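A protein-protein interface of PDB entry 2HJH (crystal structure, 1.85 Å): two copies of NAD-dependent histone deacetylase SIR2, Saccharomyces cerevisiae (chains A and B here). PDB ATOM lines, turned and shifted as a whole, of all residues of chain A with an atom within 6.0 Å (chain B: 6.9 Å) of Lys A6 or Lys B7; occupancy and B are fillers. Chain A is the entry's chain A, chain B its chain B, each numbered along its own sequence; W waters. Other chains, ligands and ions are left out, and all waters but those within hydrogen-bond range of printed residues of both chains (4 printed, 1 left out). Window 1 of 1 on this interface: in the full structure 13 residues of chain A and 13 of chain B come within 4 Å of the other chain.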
ATOM      1  N   ASP A   2      11.901 -29.167  -8.275  1.00  0.00           N
ATOM      2  CA  ASP A   2      10.837 -29.340  -9.308  1.00  0.00           C
ATOM      3  C   ASP A   2       9.788 -28.201  -9.185  1.00  0.00           C
ATOM      4  O   ASP A   2       9.526 -27.525 -10.165  1.00  0.00           O
ATOM      5  CB  ASP A   2      10.197 -30.738  -9.215  1.00  0.00           C
ATOM      6  N   PRO A   3       9.183 -27.995  -8.001  1.00  0.00           N
ATOM      7  CA  PRO A   3       8.461 -26.735  -7.739  1.00  0.00           C
ATOM      8  C   PRO A   3       9.348 -25.517  -8.020  1.00  0.00           C
ATOM      9  O   PRO A   3      10.574 -25.496  -7.733  1.00  0.00           O
ATOM     10  CB  PRO A   3       8.114 -26.795  -6.236  1.00  0.00           C
ATOM     11  CG  PRO A   3       8.163 -28.274  -5.862  1.00  0.00           C
ATOM     12  CD  PRO A   3       9.095 -28.928  -6.850  1.00  0.00           C
ATOM     13  N   LEU A   4       8.711 -24.523  -8.624  1.00  0.00           N
ATOM     14  CA  LEU A   4       9.353 -23.268  -8.928  1.00  0.00           C
ATOM     15  C   LEU A   4       9.967 -22.785  -7.613  1.00  0.00           C
ATOM     16  O   LEU A   4       9.358 -22.922  -6.525  1.00  0.00           O
ATOM     17  CB  LEU A   4       8.330 -22.268  -9.528  1.00  0.00           C
ATOM     18  CG  LEU A   4       8.777 -20.836  -9.745  1.00  0.00           C
ATOM     19  CD1 LEU A   4       9.750 -20.785 -10.900  1.00  0.00           C
ATOM     20  CD2 LEU A   4       7.574 -19.871  -9.924  1.00  0.00           C
ATOM     21  N   ALA A   5      11.211 -22.304  -7.714  1.00  0.00           N
ATOM     22  CA  ALA A   5      12.012 -21.994  -6.530  1.00  0.00           C
ATOM     23  C   ALA A   5      12.820 -20.733  -6.778  1.00  0.00           C
ATOM     24  O   ALA A   5      13.039 -20.356  -7.911  1.00  0.00           O
ATOM     25  CB  ALA A   5      12.953 -23.161  -6.208  1.00  0.00           C
ATOM     26  N   LYS A   6      13.190 -20.085  -5.681  1.00  0.00           N
ATOM     27  CA  LYS A   6      14.237 -19.077  -5.633  1.00  0.00           C
ATOM     28  C   LYS A   6      15.384 -19.504  -4.682  1.00  0.00           C
ATOM     29  O   LYS A   6      15.276 -20.480  -3.905  1.00  0.00           O
ATOM     30  CB  LYS A   6      13.674 -17.741  -5.149  1.00  0.00           C
ATOM     31  CG  LYS A   6      13.105 -17.759  -3.725  1.00  0.00           C
ATOM     32  CD  LYS A   6      12.883 -16.335  -3.190  1.00  0.00           C
ATOM     33  CE  LYS A   6      12.206 -16.320  -1.813  1.00  0.00           C
ATOM     34  NZ  LYS A   6      12.142 -14.916  -1.321  1.00  0.00           N
ATOM     35  N   LYS A   7      16.453 -18.733  -4.740  1.00  0.00           N
ATOM     36  CA  LYS A   7      17.678 -19.020  -3.997  1.00  0.00           C
ATOM     37  C   LYS A   7      17.452 -18.531  -2.573  1.00  0.00           C
ATOM     38  O   LYS A   7      16.964 -17.413  -2.354  1.00  0.00           O
ATOM     39  CB  LYS A   7      18.917 -18.306  -4.585  1.00  0.00           C
ATOM     40  CG  LYS A   7      19.441 -18.840  -5.939  1.00  0.00           C
ATOM     41  CD  LYS A   7      20.897 -18.347  -6.225  1.00  0.00           C
ATOM     42  CE  LYS A   7      21.421 -18.750  -7.620  1.00  0.00           C
ATOM     43  NZ  LYS A   7      22.957 -18.915  -7.698  1.00  0.00           N
ATOM     44  N   GLN A   8      17.794 -19.368  -1.615  1.00  0.00           N
ATOM     45  CA  GLN A   8      17.761 -18.967  -0.229  1.00  0.00           C
ATOM     46  C   GLN A   8      19.140 -19.247   0.373  1.00  0.00           C
ATOM     47  O   GLN A   8      19.609 -20.342   0.277  1.00  0.00           O
ATOM     48  CB  GLN A   8      16.758 -19.797   0.541  1.00  0.00           C
ATOM     49  CG  GLN A   8      16.758 -19.445   2.017  1.00  0.00           C
ATOM     50  CD  GLN A   8      15.646 -20.139   2.751  1.00  0.00           C
ATOM     51  OE1 GLN A   8      14.697 -19.493   3.152  1.00  0.00           O
ATOM     52  NE2 GLN A   8      15.754 -21.458   2.921  1.00  0.00           N
ATOM     53  N   ASN A 276      18.798 -31.613   1.560  1.00  0.00           N
ATOM     54  CA  ASN A 276      17.979 -30.670   0.777  1.00  0.00           C
ATOM     55  C   ASN A 276      18.672 -29.937  -0.291  1.00  0.00           C
ATOM     56  O   ASN A 276      18.004 -29.360  -1.178  1.00  0.00           O
ATOM     57  CB  ASN A 276      17.309 -29.613   1.672  1.00  0.00           C
ATOM     58  CG  ASN A 276      16.382 -30.216   2.674  1.00  0.00           C
ATOM     59  OD1 ASN A 276      15.700 -31.215   2.402  1.00  0.00           O
ATOM     60  ND2 ASN A 276      16.406 -29.667   3.878  1.00  0.00           N
ATOM     61  N   SER A 280      17.347 -33.186  -6.656  1.00  0.00           N
ATOM     62  CA  SER A 280      16.230 -34.082  -6.294  1.00  0.00           C
ATOM     63  C   SER A 280      16.362 -35.494  -6.947  1.00  0.00           C
ATOM     64  O   SER A 280      15.955 -36.504  -6.353  1.00  0.00           O
ATOM     65  CB  SER A 280      14.873 -33.349  -6.620  1.00  0.00           C
ATOM     66  OG  SER A 280      14.820 -33.245  -8.044  1.00  0.00           O
ATOM     67  N   ALA B   5      23.541 -21.398  -1.206  1.00  0.00           N
ATOM     68  CA  ALA B   5      22.079 -21.338  -1.261  1.00  0.00           C
ATOM     69  C   ALA B   5      21.516 -22.707  -1.498  1.00  0.00           C
ATOM     70  O   ALA B   5      22.183 -23.533  -2.133  1.00  0.00           O
ATOM     71  CB  ALA B   5      21.637 -20.417  -2.395  1.00  0.00           C
ATOM     72  N   LYS B   6      20.304 -22.942  -0.994  1.00  0.00           N
ATOM     73  CA  LYS B   6      19.459 -24.023  -1.457  1.00  0.00           C
ATOM     74  C   LYS B   6      18.157 -23.447  -2.144  1.00  0.00           C
ATOM     75  O   LYS B   6      17.864 -22.222  -2.071  1.00  0.00           O
ATOM     76  CB  LYS B   6      19.089 -24.936  -0.287  1.00  0.00           C
ATOM     77  CG  LYS B   6      18.274 -24.232   0.803  1.00  0.00           C
ATOM     78  CD  LYS B   6      17.456 -25.247   1.627  1.00  0.00           C
ATOM     79  CE  LYS B   6      16.814 -24.571   2.822  1.00  0.00           C
ATOM     80  NZ  LYS B   6      16.162 -25.558   3.706  1.00  0.00           N
ATOM     81  N   LYS B   7      17.409 -24.330  -2.799  1.00  0.00           N
ATOM     82  CA  LYS B   7      16.137 -23.960  -3.463  1.00  0.00           C
ATOM     83  C   LYS B   7      15.066 -23.759  -2.392  1.00  0.00           C
ATOM     84  O   LYS B   7      14.918 -24.596  -1.516  1.00  0.00           O
ATOM     85  CB  LYS B   7      15.654 -25.048  -4.419  1.00  0.00           C
ATOM     86  CG  LYS B   7      16.283 -25.029  -5.784  1.00  0.00           C
ATOM     87  CD  LYS B   7      15.341 -25.688  -6.830  1.00  0.00           C
ATOM     88  CE  LYS B   7      15.911 -26.985  -7.428  1.00  0.00           C
ATOM     89  NZ  LYS B   7      15.243 -27.331  -8.743  1.00  0.00           N
ATOM     90  N   GLN B   8      14.401 -22.617  -2.395  1.00  0.00           N
ATOM     91  CA  GLN B   8      13.256 -22.363  -1.522  1.00  0.00           C
ATOM     92  C   GLN B   8      12.035 -22.309  -2.431  1.00  0.00           C
ATOM     93  O   GLN B   8      11.958 -21.446  -3.284  1.00  0.00           O
ATOM     94  CB  GLN B   8      13.414 -21.021  -0.794  1.00  0.00           C
ATOM     95  N   THR B   9      11.104 -23.238  -2.263  1.00  0.00           N
ATOM     96  CA  THR B   9       9.921 -23.262  -3.092  1.00  0.00           C
ATOM     97  C   THR B   9       9.171 -21.929  -2.967  1.00  0.00           C
ATOM     98  O   THR B   9       9.017 -21.386  -1.857  1.00  0.00           O
ATOM     99  CB  THR B   9       9.003 -24.439  -2.766  1.00  0.00           C
ATOM    100  OG1 THR B   9       9.653 -25.682  -3.123  1.00  0.00           O
ATOM    101  CG2 THR B   9       7.769 -24.394  -3.671  1.00  0.00           C
ATOM    102  N   VAL B  10       8.800 -21.388  -4.125  1.00  0.00           N
ATOM    103  CA  VAL B  10       8.035 -20.135  -4.195  1.00  0.00           C
ATOM    104  C   VAL B  10       6.547 -20.469  -4.122  1.00  0.00           C
ATOM    105  O   VAL B  10       5.994 -21.119  -4.988  1.00  0.00           O
ATOM    106  CB  VAL B  10       8.353 -19.367  -5.460  1.00  0.00           C
ATOM    107  CG1 VAL B  10       7.420 -18.153  -5.594  1.00  0.00           C
ATOM    108  CG2 VAL B  10       9.825 -18.879  -5.415  1.00  0.00           C
ATOM    109  N   GLU B 273       8.135 -11.632  -5.992  1.00  0.00           N
ATOM    110  CA  GLU B 273       9.349 -12.441  -5.900  1.00  0.00           C
ATOM    111  C   GLU B 273      10.107 -12.548  -7.194  1.00  0.00           C
ATOM    112  O   GLU B 273      11.239 -13.090  -7.227  1.00  0.00           O
ATOM    113  CB  GLU B 273       8.988 -13.844  -5.386  1.00  0.00           C
ATOM    114  CG  GLU B 273       8.350 -13.758  -4.017  1.00  0.00           C
ATOM    115  CD  GLU B 273       9.363 -13.833  -2.893  1.00  0.00           C
ATOM    116  OE1 GLU B 273      10.576 -13.651  -3.162  1.00  0.00           O
ATOM    117  OE2 GLU B 273       8.937 -14.071  -1.741  1.00  0.00           O
ATOM    118  N   ASN B 276      13.551 -11.535  -7.071  1.00  0.00           N
ATOM    119  CA  ASN B 276      14.511 -12.410  -6.432  1.00  0.00           C
ATOM    120  C   ASN B 276      14.818 -13.641  -7.234  1.00  0.00           C
ATOM    121  O   ASN B 276      15.831 -14.288  -6.985  1.00  0.00           O
ATOM    122  CB  ASN B 276      13.988 -12.829  -5.057  1.00  0.00           C
ATOM    123  CG  ASN B 276      13.813 -11.665  -4.167  1.00  0.00           C
ATOM    124  OD1 ASN B 276      14.652 -10.756  -4.182  1.00  0.00           O
ATOM    125  ND2 ASN B 276      12.646 -11.607  -3.475  1.00  0.00           N
ATOM    126  N   MET B 277      13.944 -13.970  -8.183  1.00  0.00           N
ATOM    127  CA  MET B 277      14.052 -15.213  -8.945  1.00  0.00           C
ATOM    128  C   MET B 277      14.936 -15.065 -10.159  1.00  0.00           C
ATOM    129  O   MET B 277      15.710 -15.988 -10.502  1.00  0.00           O
ATOM    130  CB  MET B 277      12.679 -15.690  -9.389  1.00  0.00           C
ATOM    131  CG  MET B 277      11.903 -16.292  -8.276  1.00  0.00           C
ATOM    132  SD  MET B 277      10.228 -17.090  -8.847  1.00  0.00           S
ATOM    133  CE  MET B 277       9.510 -15.485  -9.500  1.00  0.00           C
HETATM  134  O   HOH W   1       6.404 -23.005  -7.134  1.00  0.00           O
HETATM  135  O   HOH W   2      14.327 -27.609   2.074  1.00  0.00           O
HETATM  136  O   HOH W   3      18.261 -27.265  -2.918  1.00  0.00           O
HETATM  137  O   HOH W   4      16.944 -16.831  -6.696  1.00  0.00           O
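O of Leu A4 lies within hydrogen-bond range of N of Val B10 (2.9 Å).
The backbone NH (N) of Gln B8 is in hydrogen-bond range of the backbone carbonyl oxygen (O) of Lys A6 (2.8 Å).
The side-chain carboxylate (OE1) of Glu B273 is in salt-bridge range of the side-chain amino group (NZ) of Lys A6.
The backbone NH (N) of Gln A8 sits at hydrogen-bond distance from the backbone carbonyl oxygen (O) of Lys B6 (2.9 Å).
Of the 9 printed residues of chain B, 9 touch a printed residue of chain A.
Hydrophobic or aromatic side chains of chain B that line the printed part of chain A: Ala B5, Val B10 and Met B277.
Among the printed residues, 19 pairs touch across the chains.
Lys B7 touches Asp A2 (NZ to N, 3.8 Å).
Thr B9 touches Pro A3 (CG2 to CB, 3.5 Å).
Thr B9 touches Leu A4 (CA to O, 3.5 Å).
Leu A4 touches Met B277.
Ala A5 touches Lys B7 (CB to CD, 3.5 Å).
Ala A5 touches Gln B8 (CA to O, 3.3 Å).
Lys B6 touches Lys A6 (O to O, 3.6 Å).
Lys B7 touches Lys A6.
Gln A8 touches Ala B5.
CB of Gln B8 touches CB of Gln A8, at 3.8 Å.
Lys A6 touches Lys B7, and with the chains exchanged Lys A7 touches Lys B6.
Lys A6 touches Gln B8, and with the chains exchanged Gln A8 touches Lys B6.
Lys A6 touches Asn B276, but with the chains exchanged Asn A276 does not touch Lys B6 (4.1 Å).
Gln A8 touches its own counterpart, Gln B8.
5 positions are printed for both chains.
Of the 19 pairs that touch across the chains among the printed residues, 8 have their exchanged pair printed and touching as well.
The side-chain carboxylate of Glu B273 lies within hydrogen-bond range of the side-chain amide nitrogen of Asn B276.
Water W3 lies within hydrogen-bond range of the backbone carbonyl oxygen of Asn A276 (2.7 Å) and the backbone NH of Lys B7 (3.1 Å).
Water W4 bridges N of Lys A7 and O of Asn B276.
Water W1 lies within hydrogen-bond range of the backbone carbonyl oxygen of Val B10 (2.9 Å) and the backbone carbonyl oxygen of Leu A4 (3.0 Å).
Water W2 lies within hydrogen-bond range of the side-chain amino group of Lys B6 (3.2 Å) and the side-chain amide nitrogen of Asn A276 (3.4 Å).
Of the printed residues of chain B, Lys A6 touches Lys B6, Lys B7, Gln B8, Val B10, Glu B273, Asn B276 and Met B277.
Of the printed residues of chain A, Lys B7 touches Asp A2 (3.8 Å), Ala A5 (3.5 Å) and Lys A6 (3.6 Å).
Of the printed residues of chain B, Leu A4 touches Thr B9, Val B10 and Met B277.
Printed residues of chain A within 4 Å of Val B10: Leu A4 (2.9 Å), Ala A5 (3.8 Å) and Lys A6 (3.6 Å).
The nearest residue of chain A that does not touch Lys B7 is Pro A3 (4.9 Å).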
